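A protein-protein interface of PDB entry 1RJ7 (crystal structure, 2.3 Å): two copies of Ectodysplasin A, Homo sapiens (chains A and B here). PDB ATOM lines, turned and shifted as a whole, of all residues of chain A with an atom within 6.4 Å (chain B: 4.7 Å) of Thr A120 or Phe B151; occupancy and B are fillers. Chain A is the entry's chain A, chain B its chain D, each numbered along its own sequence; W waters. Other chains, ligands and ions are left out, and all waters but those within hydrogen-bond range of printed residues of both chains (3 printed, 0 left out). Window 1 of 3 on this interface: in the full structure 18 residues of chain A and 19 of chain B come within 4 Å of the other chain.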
ATOM      1  N   ILE A  75      21.289   7.376   8.047  1.00  0.00           N
ATOM      2  CA  ILE A  75      22.189   6.541   8.828  1.00  0.00           C
ATOM      3  C   ILE A  75      21.954   6.863  10.288  1.00  0.00           C
ATOM      4  O   ILE A  75      21.787   8.038  10.657  1.00  0.00           O
ATOM      5  CB  ILE A  75      23.661   6.810   8.448  1.00  0.00           C
ATOM      6  CG1 ILE A  75      23.913   6.521   6.967  1.00  0.00           C
ATOM      7  CG2 ILE A  75      24.599   5.917   9.279  1.00  0.00           C
ATOM      8  CD1 ILE A  75      25.318   6.966   6.477  1.00  0.00           C
ATOM      9  N   TYR A  76      21.904   5.828  11.119  1.00  0.00           N
ATOM     10  CA  TYR A  76      21.741   6.029  12.555  1.00  0.00           C
ATOM     11  C   TYR A  76      22.531   5.034  13.399  1.00  0.00           C
ATOM     12  O   TYR A  76      22.872   3.934  12.951  1.00  0.00           O
ATOM     13  CB  TYR A  76      20.264   6.004  12.944  1.00  0.00           C
ATOM     14  CG  TYR A  76      19.594   4.658  12.801  1.00  0.00           C
ATOM     15  CD1 TYR A  76      19.643   3.711  13.832  1.00  0.00           C
ATOM     16  CD2 TYR A  76      18.892   4.337  11.657  1.00  0.00           C
ATOM     17  CE1 TYR A  76      19.018   2.472  13.714  1.00  0.00           C
ATOM     18  CE2 TYR A  76      18.271   3.104  11.521  1.00  0.00           C
ATOM     19  CZ  TYR A  76      18.327   2.178  12.555  1.00  0.00           C
ATOM     20  OH  TYR A  76      17.707   0.957  12.410  1.00  0.00           O
ATOM     21  N   SER A  77      22.803   5.437  14.635  1.00  0.00           N
ATOM     22  CA  SER A  77      23.511   4.596  15.589  1.00  0.00           C
ATOM     23  C   SER A  77      23.109   4.910  17.018  1.00  0.00           C
ATOM     24  O   SER A  77      22.639   6.014  17.341  1.00  0.00           O
ATOM     25  CB  SER A  77      25.011   4.790  15.455  1.00  0.00           C
ATOM     26  OG  SER A  77      25.369   6.127  15.741  1.00  0.00           O
ATOM     27  N   GLN A  78      23.295   3.918  17.872  1.00  0.00           N
ATOM     28  CA  GLN A  78      23.163   4.100  19.291  1.00  0.00           C
ATOM     29  C   GLN A  78      24.195   3.236  19.979  1.00  0.00           C
ATOM     30  O   GLN A  78      24.377   2.072  19.617  1.00  0.00           O
ATOM     31  CB  GLN A  78      21.756   3.746  19.762  1.00  0.00           C
ATOM     32  CG  GLN A  78      21.455   4.217  21.179  1.00  0.00           C
ATOM     33  CD  GLN A  78      20.027   3.942  21.610  1.00  0.00           C
ATOM     34  OE1 GLN A  78      19.106   4.689  21.259  1.00  0.00           O
ATOM     35  NE2 GLN A  78      19.845   2.892  22.402  1.00  0.00           N
ATOM     36  N   TYR A  92      31.799   9.208  20.061  1.00  0.00           N
ATOM     37  CA  TYR A  92      32.003   8.393  18.871  1.00  0.00           C
ATOM     38  C   TYR A  92      31.621   9.151  17.593  1.00  0.00           C
ATOM     39  O   TYR A  92      30.784  10.054  17.604  1.00  0.00           O
ATOM     40  CB  TYR A  92      31.251   7.056  18.965  1.00  0.00           C
ATOM     41  CG  TYR A  92      29.743   7.104  18.834  1.00  0.00           C
ATOM     42  CD1 TYR A  92      29.133   7.093  17.586  1.00  0.00           C
ATOM     43  CD2 TYR A  92      28.927   7.106  19.949  1.00  0.00           C
ATOM     44  CE1 TYR A  92      27.762   7.114  17.455  1.00  0.00           C
ATOM     45  CE2 TYR A  92      27.538   7.112  19.821  1.00  0.00           C
ATOM     46  CZ  TYR A  92      26.972   7.115  18.566  1.00  0.00           C
ATOM     47  OH  TYR A  92      25.608   7.140  18.423  1.00  0.00           O
ATOM     48  N   VAL A  94      30.289   8.661  13.566  1.00  0.00           N
ATOM     49  CA  VAL A  94      29.794   7.840  12.464  1.00  0.00           C
ATOM     50  C   VAL A  94      30.651   8.257  11.266  1.00  0.00           C
ATOM     51  O   VAL A  94      30.579   9.401  10.816  1.00  0.00           O
ATOM     52  CB  VAL A  94      28.277   8.055  12.239  1.00  0.00           C
ATOM     53  CG1 VAL A  94      27.771   7.317  11.004  1.00  0.00           C
ATOM     54  CG2 VAL A  94      27.505   7.557  13.443  1.00  0.00           C
ATOM     55  N   PHE A 101      31.304  11.953   9.654  1.00  0.00           N
ATOM     56  CA  PHE A 101      30.031  12.501   9.167  1.00  0.00           C
ATOM     57  C   PHE A 101      29.174  12.992  10.349  1.00  0.00           C
ATOM     58  O   PHE A 101      28.707  14.147  10.350  1.00  0.00           O
ATOM     59  CB  PHE A 101      29.277  11.445   8.329  1.00  0.00           C
ATOM     60  CG  PHE A 101      27.824  11.794   8.021  1.00  0.00           C
ATOM     61  CD1 PHE A 101      27.437  13.097   7.706  1.00  0.00           C
ATOM     62  CD2 PHE A 101      26.857  10.800   8.001  1.00  0.00           C
ATOM     63  CE1 PHE A 101      26.106  13.400   7.439  1.00  0.00           C
ATOM     64  CE2 PHE A 101      25.528  11.096   7.707  1.00  0.00           C
ATOM     65  CZ  PHE A 101      25.160  12.394   7.426  1.00  0.00           C
ATOM     66  N   LEU A 102      28.959  12.118  11.334  1.00  0.00           N
ATOM     67  CA  LEU A 102      28.264  12.494  12.568  1.00  0.00           C
ATOM     68  C   LEU A 102      29.167  12.256  13.769  1.00  0.00           C
ATOM     69  O   LEU A 102      30.050  11.396  13.743  1.00  0.00           O
ATOM     70  CB  LEU A 102      26.965  11.699  12.739  1.00  0.00           C
ATOM     71  CG  LEU A 102      26.018  11.580  11.529  1.00  0.00           C
ATOM     72  CD1 LEU A 102      25.011  10.488  11.737  1.00  0.00           C
ATOM     73  CD2 LEU A 102      25.316  12.880  11.233  1.00  0.00           C
ATOM     74  N   GLN A 103      28.954  13.040  14.815  1.00  0.00           N
ATOM     75  CA  GLN A 103      29.637  12.824  16.076  1.00  0.00           C
ATOM     76  C   GLN A 103      28.660  12.995  17.242  1.00  0.00           C
ATOM     77  O   GLN A 103      27.862  13.932  17.287  1.00  0.00           O
ATOM     78  CB  GLN A 103      30.861  13.740  16.230  1.00  0.00           C
ATOM     79  CG  GLN A 103      31.715  13.391  17.472  1.00  0.00           C
ATOM     80  CD  GLN A 103      32.979  14.203  17.619  1.00  0.00           C
ATOM     81  OE1 GLN A 103      33.279  15.061  16.798  1.00  0.00           O
ATOM     82  NE2 GLN A 103      33.730  13.930  18.683  1.00  0.00           N
ATOM     83  N   CYS A 104      28.744  12.070  18.183  1.00  0.00           N
ATOM     84  CA  CYS A 104      27.868  12.032  19.341  1.00  0.00           C
ATOM     85  C   CYS A 104      28.740  12.170  20.560  1.00  0.00           C
ATOM     86  O   CYS A 104      29.701  11.430  20.712  1.00  0.00           O
ATOM     87  CB  CYS A 104      27.151  10.675  19.380  1.00  0.00           C
ATOM     88  SG  CYS A 104      25.869  10.538  20.654  1.00  0.00           S
ATOM     89  N   CYS A 118      23.463   6.545  23.689  1.00  0.00           N
ATOM     90  CA  CYS A 118      24.001   7.684  22.962  1.00  0.00           C
ATOM     91  C   CYS A 118      23.627   7.585  21.482  1.00  0.00           C
ATOM     92  O   CYS A 118      24.282   6.863  20.702  1.00  0.00           O
ATOM     93  CB  CYS A 118      25.524   7.715  23.145  1.00  0.00           C
ATOM     94  SG  CYS A 118      26.033   7.843  24.866  1.00  0.00           S
ATOM     95  N   TYR A 119      22.571   8.311  21.113  1.00  0.00           N
ATOM     96  CA  TYR A 119      21.991   8.245  19.778  1.00  0.00           C
ATOM     97  C   TYR A 119      22.313   9.465  18.894  1.00  0.00           C
ATOM     98  O   TYR A 119      22.240  10.599  19.312  1.00  0.00           O
ATOM     99  CB  TYR A 119      20.468   8.082  19.876  1.00  0.00           C
ATOM    100  CG  TYR A 119      19.749   7.924  18.542  1.00  0.00           C
ATOM    101  CD1 TYR A 119      19.411   9.026  17.769  1.00  0.00           C
ATOM    102  CD2 TYR A 119      19.378   6.664  18.075  1.00  0.00           C
ATOM    103  CE1 TYR A 119      18.739   8.880  16.582  1.00  0.00           C
ATOM    104  CE2 TYR A 119      18.699   6.514  16.878  1.00  0.00           C
ATOM    105  CZ  TYR A 119      18.383   7.620  16.141  1.00  0.00           C
ATOM    106  OH  TYR A 119      17.717   7.478  14.960  1.00  0.00           O
ATOM    107  N   THR A 120      22.676   9.193  17.656  1.00  0.00           N
ATOM    108  CA  THR A 120      22.728  10.211  16.631  1.00  0.00           C
ATOM    109  C   THR A 120      22.294   9.633  15.286  1.00  0.00           C
ATOM    110  O   THR A 120      22.158   8.430  15.135  1.00  0.00           O
ATOM    111  CB  THR A 120      24.145  10.808  16.543  1.00  0.00           C
ATOM    112  OG1 THR A 120      24.125  11.969  15.695  1.00  0.00           O
ATOM    113  CG2 THR A 120      25.122   9.846  15.903  1.00  0.00           C
ATOM    114  N   ALA A 121      22.095  10.510  14.312  1.00  0.00           N
ATOM    115  CA  ALA A 121      21.588  10.104  13.009  1.00  0.00           C
ATOM    116  C   ALA A 121      21.582  11.282  12.041  1.00  0.00           C
ATOM    117  O   ALA A 121      21.626  12.431  12.443  1.00  0.00           O
ATOM    118  CB  ALA A 121      20.168   9.534  13.148  1.00  0.00           C
ATOM    119  N   GLY A 122      21.518  10.974  10.753  1.00  0.00           N
ATOM    120  CA  GLY A 122      21.449  11.982   9.713  1.00  0.00           C
ATOM    121  C   GLY A 122      21.487  11.409   8.307  1.00  0.00           C
ATOM    122  O   GLY A 122      21.735  10.202   8.111  1.00  0.00           O
ATOM    123  N   HIS B  24      20.860  18.284   4.680  1.00  0.00           N
ATOM    124  CA  HIS B  24      21.601  18.135   5.927  1.00  0.00           C
ATOM    125  C   HIS B  24      22.469  19.346   6.121  1.00  0.00           C
ATOM    126  O   HIS B  24      23.445  19.515   5.437  1.00  0.00           O
ATOM    127  CB  HIS B  24      22.458  16.870   5.898  1.00  0.00           C
ATOM    128  CG  HIS B  24      23.139  16.566   7.193  1.00  0.00           C
ATOM    129  ND1 HIS B  24      22.481  16.009   8.265  1.00  0.00           N
ATOM    130  CD2 HIS B  24      24.430  16.716   7.579  1.00  0.00           C
ATOM    131  CE1 HIS B  24      23.326  15.863   9.266  1.00  0.00           C
ATOM    132  NE2 HIS B  24      24.519  16.270   8.873  1.00  0.00           N
ATOM    133  N   LEU B  25      22.082  20.207   7.043  1.00  0.00           N
ATOM    134  CA  LEU B  25      22.859  21.397   7.380  1.00  0.00           C
ATOM    135  C   LEU B  25      23.752  21.096   8.576  1.00  0.00           C
ATOM    136  O   LEU B  25      23.360  20.384   9.510  1.00  0.00           O
ATOM    137  CB  LEU B  25      21.944  22.575   7.711  1.00  0.00           C
ATOM    138  CG  LEU B  25      20.787  22.854   6.735  1.00  0.00           C
ATOM    139  CD1 LEU B  25      19.802  23.816   7.372  1.00  0.00           C
ATOM    140  CD2 LEU B  25      21.279  23.387   5.395  1.00  0.00           C
ATOM    141  N   GLN B  26      24.956  21.653   8.532  1.00  0.00           N
ATOM    142  CA  GLN B  26      26.003  21.393   9.507  1.00  0.00           C
ATOM    143  C   GLN B  26      26.482  22.729  10.055  1.00  0.00           C
ATOM    144  O   GLN B  26      26.390  23.753   9.381  1.00  0.00           O
ATOM    145  CB  GLN B  26      27.188  20.670   8.833  1.00  0.00           C
ATOM    146  CG  GLN B  26      26.875  19.257   8.302  1.00  0.00           C
ATOM    147  CD  GLN B  26      28.080  18.562   7.635  1.00  0.00           C
ATOM    148  OE1 GLN B  26      28.875  19.203   6.947  1.00  0.00           O
ATOM    149  NE2 GLN B  26      28.192  17.249   7.822  1.00  0.00           N
ATOM    150  N   TRP B  46      24.445  28.033   9.409  1.00  0.00           N
ATOM    151  CA  TRP B  46      24.363  26.699   8.836  1.00  0.00           C
ATOM    152  C   TRP B  46      25.132  26.663   7.516  1.00  0.00           C
ATOM    153  O   TRP B  46      25.042  27.588   6.702  1.00  0.00           O
ATOM    154  CB  TRP B  46      22.923  26.300   8.598  1.00  0.00           C
ATOM    155  CG  TRP B  46      22.131  26.119   9.836  1.00  0.00           C
ATOM    156  CD1 TRP B  46      21.041  26.828  10.207  1.00  0.00           C
ATOM    157  CD2 TRP B  46      22.362  25.158  10.881  1.00  0.00           C
ATOM    158  NE1 TRP B  46      20.571  26.375  11.412  1.00  0.00           N
ATOM    159  CE2 TRP B  46      21.358  25.347  11.850  1.00  0.00           C
ATOM    160  CE3 TRP B  46      23.311  24.146  11.090  1.00  0.00           C
ATOM    161  CZ2 TRP B  46      21.267  24.567  13.012  1.00  0.00           C
ATOM    162  CZ3 TRP B  46      23.220  23.362  12.262  1.00  0.00           C
ATOM    163  CH2 TRP B  46      22.214  23.587  13.200  1.00  0.00           C
ATOM    164  N   TYR B  76      14.976  16.490  11.662  1.00  0.00           N
ATOM    165  CA  TYR B  76      15.866  16.176  12.780  1.00  0.00           C
ATOM    166  C   TYR B  76      16.834  17.304  13.071  1.00  0.00           C
ATOM    167  O   TYR B  76      17.031  18.212  12.258  1.00  0.00           O
ATOM    168  CB  TYR B  76      16.648  14.887  12.524  1.00  0.00           C
ATOM    169  CG  TYR B  76      17.615  14.931  11.368  1.00  0.00           C
ATOM    170  CD1 TYR B  76      17.207  14.577  10.099  1.00  0.00           C
ATOM    171  CD2 TYR B  76      18.957  15.300  11.553  1.00  0.00           C
ATOM    172  CE1 TYR B  76      18.097  14.589   9.042  1.00  0.00           C
ATOM    173  CE2 TYR B  76      19.857  15.317  10.495  1.00  0.00           C
ATOM    174  CZ  TYR B  76      19.413  14.955   9.247  1.00  0.00           C
ATOM    175  OH  TYR B  76      20.247  14.972   8.173  1.00  0.00           O
ATOM    176  N   SER B  77      17.418  17.236  14.256  1.00  0.00           N
ATOM    177  CA  SER B  77      18.372  18.236  14.716  1.00  0.00           C
ATOM    178  C   SER B  77      19.230  17.689  15.846  1.00  0.00           C
ATOM    179  O   SER B  77      18.786  16.891  16.661  1.00  0.00           O
ATOM    180  CB  SER B  77      17.662  19.484  15.206  1.00  0.00           C
ATOM    181  OG  SER B  77      16.837  19.200  16.345  1.00  0.00           O
ATOM    182  N   GLN B  78      20.470  18.141  15.874  1.00  0.00           N
ATOM    183  CA  GLN B  78      21.377  17.850  16.960  1.00  0.00           C
ATOM    184  C   GLN B  78      22.140  19.120  17.281  1.00  0.00           C
ATOM    185  O   GLN B  78      22.703  19.740  16.388  1.00  0.00           O
ATOM    186  CB  GLN B  78      22.332  16.736  16.560  1.00  0.00           C
ATOM    187  CG  GLN B  78      23.182  16.275  17.702  1.00  0.00           C
ATOM    188  CD  GLN B  78      24.095  15.134  17.339  1.00  0.00           C
ATOM    189  OE1 GLN B  78      23.668  13.978  17.282  1.00  0.00           O
ATOM    190  NE2 GLN B  78      25.354  15.448  17.101  1.00  0.00           N
ATOM    191  N   TYR B 119      19.986  15.492  20.666  1.00  0.00           N
ATOM    192  CA  TYR B 119      19.337  15.116  19.399  1.00  0.00           C
ATOM    193  C   TYR B 119      17.835  14.914  19.547  1.00  0.00           C
ATOM    194  O   TYR B 119      17.365  14.337  20.522  1.00  0.00           O
ATOM    195  CB  TYR B 119      19.940  13.808  18.850  1.00  0.00           C
ATOM    196  CG  TYR B 119      19.330  13.315  17.524  1.00  0.00           C
ATOM    197  CD1 TYR B 119      18.106  12.646  17.507  1.00  0.00           C
ATOM    198  CD2 TYR B 119      19.991  13.487  16.316  1.00  0.00           C
ATOM    199  CE1 TYR B 119      17.540  12.191  16.349  1.00  0.00           C
ATOM    200  CE2 TYR B 119      19.435  13.014  15.120  1.00  0.00           C
ATOM    201  CZ  TYR B 119      18.199  12.366  15.153  1.00  0.00           C
ATOM    202  OH  TYR B 119      17.593  11.910  14.012  1.00  0.00           O
ATOM    203  N   HIS B 148      30.228  18.333  12.715  1.00  0.00           N
ATOM    204  CA  HIS B 148      29.762  16.961  12.925  1.00  0.00           C
ATOM    205  C   HIS B 148      28.810  16.777  14.113  1.00  0.00           C
ATOM    206  O   HIS B 148      27.972  15.845  14.118  1.00  0.00           O
ATOM    207  CB  HIS B 148      30.977  16.045  13.075  1.00  0.00           C
ATOM    208  CG  HIS B 148      31.973  16.162  11.958  1.00  0.00           C
ATOM    209  ND1 HIS B 148      31.646  15.912  10.641  1.00  0.00           N
ATOM    210  CD2 HIS B 148      33.289  16.484  11.964  1.00  0.00           C
ATOM    211  CE1 HIS B 148      32.717  16.076   9.887  1.00  0.00           C
ATOM    212  NE2 HIS B 148      33.729  16.415  10.665  1.00  0.00           N
ATOM    213  N   THR B 149      28.897  17.682  15.093  1.00  0.00           N
ATOM    214  CA  THR B 149      28.172  17.548  16.375  1.00  0.00           C
ATOM    215  C   THR B 149      26.917  18.401  16.486  1.00  0.00           C
ATOM    216  O   THR B 149      26.059  18.131  17.346  1.00  0.00           O
ATOM    217  CB  THR B 149      29.091  17.864  17.572  1.00  0.00           C
ATOM    218  OG1 THR B 149      29.429  19.256  17.584  1.00  0.00           O
ATOM    219  CG2 THR B 149      30.413  17.145  17.458  1.00  0.00           C
ATOM    220  N   THR B 150      26.823  19.435  15.645  1.00  0.00           N
ATOM    221  CA  THR B 150      25.624  20.274  15.555  1.00  0.00           C
ATOM    222  C   THR B 150      25.122  20.321  14.111  1.00  0.00           C
ATOM    223  O   THR B 150      25.815  20.782  13.210  1.00  0.00           O
ATOM    224  CB  THR B 150      25.913  21.687  16.046  1.00  0.00           C
ATOM    225  OG1 THR B 150      26.186  21.651  17.452  1.00  0.00           O
ATOM    226  CG2 THR B 150      24.688  22.570  15.938  1.00  0.00           C
ATOM    227  N   PHE B 151      23.919  19.817  13.900  1.00  0.00           N
ATOM    228  CA  PHE B 151      23.376  19.716  12.567  1.00  0.00           C
ATOM    229  C   PHE B 151      21.856  19.814  12.599  1.00  0.00           C
ATOM    230  O   PHE B 151      21.238  19.879  13.664  1.00  0.00           O
ATOM    231  CB  PHE B 151      23.910  18.458  11.835  1.00  0.00           C
ATOM    232  CG  PHE B 151      23.715  17.159  12.575  1.00  0.00           C
ATOM    233  CD1 PHE B 151      22.459  16.552  12.638  1.00  0.00           C
ATOM    234  CD2 PHE B 151      24.785  16.521  13.168  1.00  0.00           C
ATOM    235  CE1 PHE B 151      22.281  15.331  13.318  1.00  0.00           C
ATOM    236  CE2 PHE B 151      24.614  15.291  13.855  1.00  0.00           C
ATOM    237  CZ  PHE B 151      23.368  14.705  13.923  1.00  0.00           C
ATOM    238  N   PHE B 152      21.270  19.875  11.413  1.00  0.00           N
ATOM    239  CA  PHE B 152      19.876  20.257  11.231  1.00  0.00           C
ATOM    240  C   PHE B 152      19.509  19.768   9.839  1.00  0.00           C
ATOM    241  O   PHE B 152      20.185  20.096   8.877  1.00  0.00           O
ATOM    242  CB  PHE B 152      19.755  21.776  11.320  1.00  0.00           C
ATOM    243  CG  PHE B 152      18.359  22.305  11.142  1.00  0.00           C
ATOM    244  CD1 PHE B 152      17.246  21.536  11.446  1.00  0.00           C
ATOM    245  CD2 PHE B 152      18.164  23.600  10.697  1.00  0.00           C
ATOM    246  CE1 PHE B 152      15.994  22.026  11.273  1.00  0.00           C
ATOM    247  CE2 PHE B 152      16.900  24.101  10.541  1.00  0.00           C
ATOM    248  CZ  PHE B 152      15.811  23.318  10.835  1.00  0.00           C
ATOM    249  N   GLY B 153      18.476  18.954   9.733  1.00  0.00           N
ATOM    250  CA  GLY B 153      18.204  18.257   8.489  1.00  0.00           C
ATOM    251  C   GLY B 153      16.759  17.882   8.269  1.00  0.00           C
ATOM    252  O   GLY B 153      15.919  18.083   9.137  1.00  0.00           O
HETATM  253  O   HOH W   1      23.374  13.206  19.962  1.00  0.00           O
HETATM  254  O   HOH W   2      27.322  16.200   9.962  1.00  0.00           O
HETATM  255  O   HOH W   3      16.294   9.597  14.381  1.00  0.00           O
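The side-chain amide oxygen (OE1) of Gln B78 lies within hydrogen-bond range of the side-chain hydroxyl (OG1) of Thr A120 (2.6 Å). The backbone carbonyl oxygen (O) of Phe A101 is in hydrogen-bond range of a ring nitrogen (ND1) of His B148 (3.4 Å). The backbone carbonyl oxygen of His B148 sits at hydrogen-bond distance from the backbone NH of Gln A103 (3.1 Å). The side-chain amide nitrogen (NE2) of Gln B78 lies within hydrogen-bond range of the backbone carbonyl oxygen (O) of Gln A103 (2.9 Å).
N of Val A94 is in hydrogen-bond range of O of Leu A102. The backbone NH (N) of Ile A75 is in hydrogen-bond range of the backbone carbonyl oxygen (O) of Gly A122 (2.9 Å). N of Phe B151 is in hydrogen-bond range of O of Gln B78 (2.8 Å). The backbone carbonyl oxygen of Tyr B76 sits at hydrogen-bond distance from the backbone NH of Gly B153 (3.0 Å). The backbone NH of Ser A77 sits at hydrogen-bond distance from the backbone carbonyl oxygen of Thr A120, 3.1 Å away. O of Thr B149 lies within hydrogen-bond range of NE2 of Gln B78.
NE2 of His B24 touches CE1 of Phe A101 (3.6 Å). Leu A102 touches His B148 (CA to O, 3.7 Å). CD2 of Leu A102 touches CE2 of Phe B151, 3.6 Å away. Thr B149 touches Gln A103 (CG2 to OE1, 3.6 Å). CE1 of Tyr A119 touches CE1 of Tyr B119, at 3.5 Å. CZ of Phe B151 touches OG1 of Thr A120, 3.3 Å away. Ala A121 touches Tyr B76. Ala A121 touches Tyr B119 (O to CE2, 3.5 Å). CE1 of Phe B151 touches O of Ala A121, at 3.1 Å. Gly A122 touches Tyr B76.
Printed residues of chain B within 4 Å of Phe A101: His B24 and His B148. Cys A118 touches none of the printed residues of chain B. Printed residues of chain B within 4 Å of Tyr A119: Tyr B119. Thr A120 touches just these residues of chain B: Gln B78 and Phe B151. Printed residues of chain B within 4 Å of Gly A122: Tyr B76. Of the printed residues of chain A, His B24 touches Phe A101 (3.6 Å). Gln B26 touches none of the printed residues of chain A. Of the printed residues of chain A, Thr B149 touches Gln A103 (3.6 Å). The nearest residue of chain B that does not touch Thr A120 is Tyr B119 (4.3 Å). The nearest residue of chain A that does not touch Phe B151 is Gln A103 (4.9 Å). The nearest printed residue of chain A that does not touch Thr B149 is Cys A104 (5.4 Å).
Of the 15 printed residues of chain A, 7 touch a printed residue of chain B. Printed residues of chain A that touch a printed residue of chain B: Phe A101, Leu A102, Gln A103, Tyr A119, Thr A120, Ala A121 and Gly A122. Hydrophobic or aromatic side chains of chain A within 4 Å of the printed part of chain B: Phe A101, Leu A102, Tyr A119 and Ala A121. Hydrophobic or aromatic side chains of chain B that line the printed part of chain A: His B24, Tyr B76, Tyr B119, His B148 and Phe B151. Among the printed residues, no Asp or Glu carboxylate lies within 4 Å of a Lys or Arg side-chain nitrogen of the other chain.
Tyr B119 touches its own counterpart, Tyr A119. 4 positions are printed for both chains. Of the 14 pairs that touch across the chains among the printed residues, 1 has its exchanged pair printed and touching as well.
Water W2 lies within hydrogen-bond range of O of Phe A101 (2.5 Å), NE2 of Gln B26 (2.5 Å) and NE2 of His B24 (3.0 Å). Water W3 bridges OH of Tyr A119 and OH of Tyr B119. Water W1 lies within hydrogen-bond range of the side-chain amide oxygen of Gln B78 (2.8 Å), the backbone carbonyl oxygen of Tyr A119 (2.9 Å) and the side-chain sulfur of Cys A104 (3.7 Å).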
